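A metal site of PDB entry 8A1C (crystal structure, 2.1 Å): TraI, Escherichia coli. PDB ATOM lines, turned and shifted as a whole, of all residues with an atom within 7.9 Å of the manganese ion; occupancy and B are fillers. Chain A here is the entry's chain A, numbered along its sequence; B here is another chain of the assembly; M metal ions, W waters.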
ATOM      1  N   SER A  14      25.925   4.965  10.444  1.00  0.00           N
ATOM      2  CA  SER A  14      26.167   4.375   9.131  1.00  0.00           C
ATOM      3  C   SER A  14      24.870   4.104   8.382  1.00  0.00           C
ATOM      4  O   SER A  14      24.924   3.774   7.195  1.00  0.00           O
ATOM      5  CB  SER A  14      26.958   3.079   9.275  1.00  0.00           C
ATOM      6  OG  SER A  14      28.129   3.270  10.058  1.00  0.00           O
ATOM      7  N   GLY A  17      21.922   6.902   5.492  1.00  0.00           N
ATOM      8  CA  GLY A  17      21.704   6.958   4.067  1.00  0.00           C
ATOM      9  C   GLY A  17      20.800   5.889   3.476  1.00  0.00           C
ATOM     10  O   GLY A  17      20.675   5.823   2.252  1.00  0.00           O
ATOM     11  N   TYR A  18      20.161   5.058   4.306  1.00  0.00           N
ATOM     12  CA  TYR A  18      19.375   3.959   3.754  1.00  0.00           C
ATOM     13  C   TYR A  18      18.299   4.453   2.797  1.00  0.00           C
ATOM     14  O   TYR A  18      17.999   3.795   1.800  1.00  0.00           O
ATOM     15  CB  TYR A  18      18.738   3.148   4.884  1.00  0.00           C
ATOM     16  CG  TYR A  18      19.617   2.052   5.458  1.00  0.00           C
ATOM     17  CD1 TYR A  18      20.974   1.981   5.166  1.00  0.00           C
ATOM     18  CD2 TYR A  18      19.071   1.079   6.291  1.00  0.00           C
ATOM     19  CE1 TYR A  18      21.761   0.971   5.690  1.00  0.00           C
ATOM     20  CE2 TYR A  18      19.853   0.086   6.828  1.00  0.00           C
ATOM     21  CZ  TYR A  18      21.191   0.023   6.526  1.00  0.00           C
ATOM     22  OH  TYR A  18      21.952  -0.989   7.066  1.00  0.00           O
ATOM     23  N   ASP A  21      20.265   7.518  -0.114  1.00  0.00           N
ATOM     24  CA  ASP A  21      21.171   6.992  -1.124  1.00  0.00           C
ATOM     25  C   ASP A  21      20.454   6.428  -2.343  1.00  0.00           C
ATOM     26  O   ASP A  21      21.123   6.090  -3.317  1.00  0.00           O
ATOM     27  CB  ASP A  21      22.058   5.891  -0.518  1.00  0.00           C
ATOM     28  CG  ASP A  21      23.235   6.441   0.258  1.00  0.00           C
ATOM     29  OD1 ASP A  21      23.281   7.674   0.498  1.00  0.00           O
ATOM     30  OD2 ASP A  21      24.106   5.641   0.653  1.00  0.00           O
ATOM     31  N   ALA A  22      19.137   6.315  -2.301  1.00  0.00           N
ATOM     32  CA  ALA A  22      18.372   5.723  -3.388  1.00  0.00           C
ATOM     33  C   ALA A  22      17.581   6.740  -4.195  1.00  0.00           C
ATOM     34  O   ALA A  22      16.899   6.365  -5.156  1.00  0.00           O
ATOM     35  CB  ALA A  22      17.418   4.650  -2.844  1.00  0.00           C
ATOM     36  N   ASP A  84      23.319  -5.683   9.443  1.00  0.00           N
ATOM     37  CA  ASP A  84      23.209  -5.345   8.036  1.00  0.00           C
ATOM     38  C   ASP A  84      23.752  -6.504   7.204  1.00  0.00           C
ATOM     39  O   ASP A  84      24.961  -6.752   7.193  1.00  0.00           O
ATOM     40  CB  ASP A  84      23.963  -4.060   7.728  1.00  0.00           C
ATOM     41  CG  ASP A  84      23.793  -3.607   6.292  1.00  0.00           C
ATOM     42  OD1 ASP A  84      23.417  -4.440   5.440  1.00  0.00           O
ATOM     43  OD2 ASP A  84      24.023  -2.410   6.013  1.00  0.00           O
ATOM     44  N   THR A  86      24.389  -7.305   3.701  1.00  0.00           N
ATOM     45  CA  THR A  86      24.507  -6.648   2.401  1.00  0.00           C
ATOM     46  C   THR A  86      24.779  -7.686   1.323  1.00  0.00           C
ATOM     47  O   THR A  86      25.857  -8.295   1.304  1.00  0.00           O
ATOM     48  CB  THR A  86      25.604  -5.599   2.411  1.00  0.00           C
ATOM     49  OG1 THR A  86      25.483  -4.769   3.562  1.00  0.00           O
ATOM     50  CG2 THR A  86      25.524  -4.743   1.154  1.00  0.00           C
ATOM     51  N   PHE A 147      16.763  -2.689   1.868  1.00  0.00           N
ATOM     52  CA  PHE A 147      16.968  -1.411   1.203  1.00  0.00           C
ATOM     53  C   PHE A 147      17.897  -1.636   0.012  1.00  0.00           C
ATOM     54  O   PHE A 147      19.047  -2.040   0.198  1.00  0.00           O
ATOM     55  CB  PHE A 147      17.583  -0.367   2.147  1.00  0.00           C
ATOM     56  CG  PHE A 147      16.732  -0.049   3.343  1.00  0.00           C
ATOM     57  CD1 PHE A 147      16.771  -0.841   4.479  1.00  0.00           C
ATOM     58  CD2 PHE A 147      15.897   1.058   3.340  1.00  0.00           C
ATOM     59  CE1 PHE A 147      15.998  -0.543   5.588  1.00  0.00           C
ATOM     60  CE2 PHE A 147      15.120   1.360   4.442  1.00  0.00           C
ATOM     61  CZ  PHE A 147      15.174   0.560   5.563  1.00  0.00           C
ATOM     62  N   ARG A 148      17.402  -1.360  -1.188  1.00  0.00           N
ATOM     63  CA  ARG A 148      18.156  -1.597  -2.421  1.00  0.00           C
ATOM     64  C   ARG A 148      18.800  -0.318  -2.914  1.00  0.00           C
ATOM     65  O   ARG A 148      18.106   0.685  -3.145  1.00  0.00           O
ATOM     66  CB  ARG A 148      17.248  -2.170  -3.512  1.00  0.00           C
ATOM     67  CG  ARG A 148      17.985  -2.519  -4.786  1.00  0.00           C
ATOM     68  CD  ARG A 148      17.056  -3.126  -5.818  1.00  0.00           C
ATOM     69  NE  ARG A 148      16.156  -2.134  -6.399  1.00  0.00           N
ATOM     70  CZ  ARG A 148      14.841  -2.274  -6.494  1.00  0.00           C
ATOM     71  NH1 ARG A 148      14.212  -3.345  -6.048  1.00  0.00           N
ATOM     72  NH2 ARG A 148      14.127  -1.295  -7.056  1.00  0.00           N
ATOM     73  N   HIS A 149      20.113  -0.354  -3.118  1.00  0.00           N
ATOM     74  CA  HIS A 149      20.873   0.779  -3.611  1.00  0.00           C
ATOM     75  C   HIS A 149      21.623   0.395  -4.887  1.00  0.00           C
ATOM     76  O   HIS A 149      21.869  -0.781  -5.160  1.00  0.00           O
ATOM     77  CB  HIS A 149      21.882   1.278  -2.574  1.00  0.00           C
ATOM     78  CG  HIS A 149      21.246   1.768  -1.309  1.00  0.00           C
ATOM     79  ND1 HIS A 149      21.930   1.810  -0.108  1.00  0.00           N
ATOM     80  CD2 HIS A 149      20.015   2.255  -1.052  1.00  0.00           C
ATOM     81  CE1 HIS A 149      21.136   2.291   0.830  1.00  0.00           C
ATOM     82  NE2 HIS A 149      19.972   2.568   0.290  1.00  0.00           N
ATOM     83  N   GLU A 150      22.008   1.425  -5.652  1.00  0.00           N
ATOM     84  CA  GLU A 150      22.637   1.232  -6.952  1.00  0.00           C
ATOM     85  C   GLU A 150      24.051   1.767  -7.058  1.00  0.00           C
ATOM     86  O   GLU A 150      24.699   1.551  -8.093  1.00  0.00           O
ATOM     87  CB  GLU A 150      21.791   1.890  -8.051  1.00  0.00           C
ATOM     88  CG  GLU A 150      20.472   1.202  -8.316  1.00  0.00           C
ATOM     89  CD  GLU A 150      19.616   1.956  -9.302  1.00  0.00           C
ATOM     90  OE1 GLU A 150      20.056   3.031  -9.771  1.00  0.00           O
ATOM     91  OE2 GLU A 150      18.500   1.482  -9.611  1.00  0.00           O
ATOM     92  N   THR A 151      24.551   2.482  -6.049  1.00  0.00           N
ATOM     93  CA  THR A 151      25.851   3.132  -6.136  1.00  0.00           C
ATOM     94  C   THR A 151      26.718   2.732  -4.952  1.00  0.00           C
ATOM     95  O   THR A 151      26.219   2.405  -3.866  1.00  0.00           O
ATOM     96  CB  THR A 151      25.717   4.658  -6.166  1.00  0.00           C
ATOM     97  OG1 THR A 151      25.223   5.119  -4.901  1.00  0.00           O
ATOM     98  CG2 THR A 151      24.778   5.091  -7.271  1.00  0.00           C
ATOM     99  N   SER A 152      28.031   2.737  -5.172  1.00  0.00           N
ATOM    100  CA  SER A 152      28.991   2.507  -4.106  1.00  0.00           C
ATOM    101  C   SER A 152      29.443   3.847  -3.520  1.00  0.00           C
ATOM    102  O   SER A 152      29.114   4.926  -4.029  1.00  0.00           O
ATOM    103  CB  SER A 152      30.189   1.725  -4.632  1.00  0.00           C
ATOM    104  OG  SER A 152      31.162   2.585  -5.207  1.00  0.00           O
ATOM    105  N   ARG A 153      30.206   3.781  -2.433  1.00  0.00           N
ATOM    106  CA  ARG A 153      30.695   4.992  -1.800  1.00  0.00           C
ATOM    107  C   ARG A 153      31.650   5.774  -2.712  1.00  0.00           C
ATOM    108  O   ARG A 153      31.827   6.975  -2.508  1.00  0.00           O
ATOM    109  CB  ARG A 153      31.386   4.673  -0.471  1.00  0.00           C
ATOM    110  CG  ARG A 153      30.463   4.050   0.592  1.00  0.00           C
ATOM    111  CD  ARG A 153      29.382   5.024   1.063  1.00  0.00           C
ATOM    112  NE  ARG A 153      28.519   4.427   2.091  1.00  0.00           N
ATOM    113  CZ  ARG A 153      27.380   4.956   2.510  1.00  0.00           C
ATOM    114  NH1 ARG A 153      26.909   6.098   2.023  1.00  0.00           N
ATOM    115  NH2 ARG A 153      26.672   4.316   3.442  1.00  0.00           N
ATOM    116  N   ASP A 158      26.961  -0.234  -8.332  1.00  0.00           N
ATOM    117  CA  ASP A 158      27.062  -1.367  -7.407  1.00  0.00           C
ATOM    118  C   ASP A 158      25.658  -1.706  -6.929  1.00  0.00           C
ATOM    119  O   ASP A 158      25.175  -1.111  -5.962  1.00  0.00           O
ATOM    120  CB  ASP A 158      27.981  -1.038  -6.228  1.00  0.00           C
ATOM    121  CG  ASP A 158      28.259  -2.245  -5.366  1.00  0.00           C
ATOM    122  OD1 ASP A 158      28.276  -2.101  -4.120  1.00  0.00           O
ATOM    123  OD2 ASP A 158      28.475  -3.344  -5.917  1.00  0.00           O
ATOM    124  N   HIS A 160      23.225  -3.471  -4.852  1.00  0.00           N
ATOM    125  CA  HIS A 160      23.259  -4.204  -3.599  1.00  0.00           C
ATOM    126  C   HIS A 160      22.017  -3.857  -2.785  1.00  0.00           C
ATOM    127  O   HIS A 160      21.390  -2.819  -2.998  1.00  0.00           O
ATOM    128  CB  HIS A 160      24.525  -3.873  -2.796  1.00  0.00           C
ATOM    129  CG  HIS A 160      24.590  -2.448  -2.325  1.00  0.00           C
ATOM    130  ND1 HIS A 160      25.185  -1.456  -3.073  1.00  0.00           N
ATOM    131  CD2 HIS A 160      24.136  -1.856  -1.193  1.00  0.00           C
ATOM    132  CE1 HIS A 160      25.098  -0.308  -2.416  1.00  0.00           C
ATOM    133  NE2 HIS A 160      24.472  -0.523  -1.276  1.00  0.00           N
ATOM    134  N   THR A 161      21.679  -4.754  -1.868  1.00  0.00           N
ATOM    135  CA  THR A 161      20.547  -4.569  -0.966  1.00  0.00           C
ATOM    136  C   THR A 161      21.019  -4.722   0.464  1.00  0.00           C
ATOM    137  O   THR A 161      21.711  -5.692   0.795  1.00  0.00           O
ATOM    138  CB  THR A 161      19.432  -5.576  -1.257  1.00  0.00           C
ATOM    139  OG1 THR A 161      18.848  -5.316  -2.529  1.00  0.00           O
ATOM    140  CG2 THR A 161      18.346  -5.487  -0.190  1.00  0.00           C
ATOM    141  N   HIS A 162      20.649  -3.760   1.310  1.00  0.00           N
ATOM    142  CA  HIS A 162      20.882  -3.851   2.757  1.00  0.00           C
ATOM    143  C   HIS A 162      19.696  -4.602   3.359  1.00  0.00           C
ATOM    144  O   HIS A 162      18.601  -4.050   3.461  1.00  0.00           O
ATOM    145  CB  HIS A 162      21.022  -2.461   3.371  1.00  0.00           C
ATOM    146  CG  HIS A 162      22.168  -1.660   2.824  1.00  0.00           C
ATOM    147  ND1 HIS A 162      23.442  -1.756   3.334  1.00  0.00           N
ATOM    148  CD2 HIS A 162      22.221  -0.732   1.841  1.00  0.00           C
ATOM    149  CE1 HIS A 162      24.241  -0.935   2.675  1.00  0.00           C
ATOM    150  NE2 HIS A 162      23.527  -0.296   1.758  1.00  0.00           N
ATOM    151  P    DT B  11      31.974   0.242  -0.071  1.00  0.00           P
ATOM    152  OP1  DT B  11      31.138   1.348  -0.588  1.00  0.00           O
ATOM    153  OP2  DT B  11      32.841   0.470   1.108  1.00  0.00           O
ATOM    154  O5'  DT B  11      30.998  -0.953   0.285  1.00  0.00           O
ATOM    155  C5'  DT B  11      29.873  -0.675   1.051  1.00  0.00           C
ATOM    156  C4'  DT B  11      28.771  -1.658   0.727  1.00  0.00           C
ATOM    157  O4'  DT B  11      29.208  -3.000   1.054  1.00  0.00           O
ATOM    158  C3'  DT B  11      27.498  -1.437   1.513  1.00  0.00           C
ATOM    159  O3'  DT B  11      26.366  -1.765   0.720  1.00  0.00           O
ATOM    160  C2'  DT B  11      27.653  -2.347   2.732  1.00  0.00           C
ATOM    161  C1'  DT B  11      28.633  -3.429   2.275  1.00  0.00           C
ATOM    162  N1   DT B  11      29.729  -3.681   3.255  1.00  0.00           N
ATOM    163  C2   DT B  11      29.464  -4.427   4.372  1.00  0.00           C
ATOM    164  O2   DT B  11      28.361  -4.909   4.616  1.00  0.00           O
ATOM    165  N3   DT B  11      30.532  -4.610   5.213  1.00  0.00           N
ATOM    166  C4   DT B  11      31.817  -4.119   5.042  1.00  0.00           C
ATOM    167  O4   DT B  11      32.709  -4.334   5.857  1.00  0.00           O
ATOM    168  C5   DT B  11      32.024  -3.339   3.850  1.00  0.00           C
ATOM    169  C7   DT B  11      33.372  -2.762   3.559  1.00  0.00           C
ATOM    170  C6   DT B  11      30.983  -3.164   3.014  1.00  0.00           C
HETATM  171 MN    MN M   1      24.020   1.072   0.252  1.00  0.00          MN
HETATM  172  O   HOH W   1      24.233   3.464   2.681  1.00  0.00           O
HETATM  173  O   HOH W   2      24.780   2.692  -0.893  1.00  0.00           O
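NE2 of His 162 sits close to O3' of DT 11 of chain B (3.4 Å).
The backbone carbonyl oxygen (O) of Phe 147 sits at hydrogen-bond distance from the backbone NH (N) of His 162, at 2.6 Å.
The side-chain carboxylate (OD2) of Asp 84 is in hydrogen-bond range of a ring nitrogen (ND1) of His 162 (2.8 Å).
A ring nitrogen (NE2) of His 149 sits at hydrogen-bond distance from the backbone carbonyl oxygen (O) of Tyr 18.
NE2 of His 160 lies close to O3' of DT 11 of chain B, 3.0 Å away.
A ring nitrogen (ND1) of His 160 sits at hydrogen-bond distance from the backbone carbonyl oxygen (O) of Asp 158 (2.9 Å).
OP1 of DT 11 of chain B lies close to the backbone NH (N) of Arg 153.
O2 of DT 11 of chain B sits at hydrogen-bond distance from the side-chain hydroxyl of Thr 86 (3.1 Å).
Water W2 lies within hydrogen-bond range of the backbone carbonyl oxygen of Thr 151 (3.3 Å) and the side-chain carboxylate of Asp 21 (3.4 Å).
Water W1 bridges NH2 of Arg 153 (2.7 Å) and OD2 of Asp 21 (3.0 Å).
O3' of DT 11 of chain B touches the manganese ion, at 3.7 Å.
Four residues have an atom within 4 Å of the manganese ion: His 149, His 160, His 162 and DT 11 of chain B.
The manganese ion is bound by NE2 of His 162 (2.1 Å), water W2 (2.1 Å), ND1 of His 149 (2.2 Å) and NE2 of His 160 (2.3 Å).
The manganese ion has four donor atoms within binding distance.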
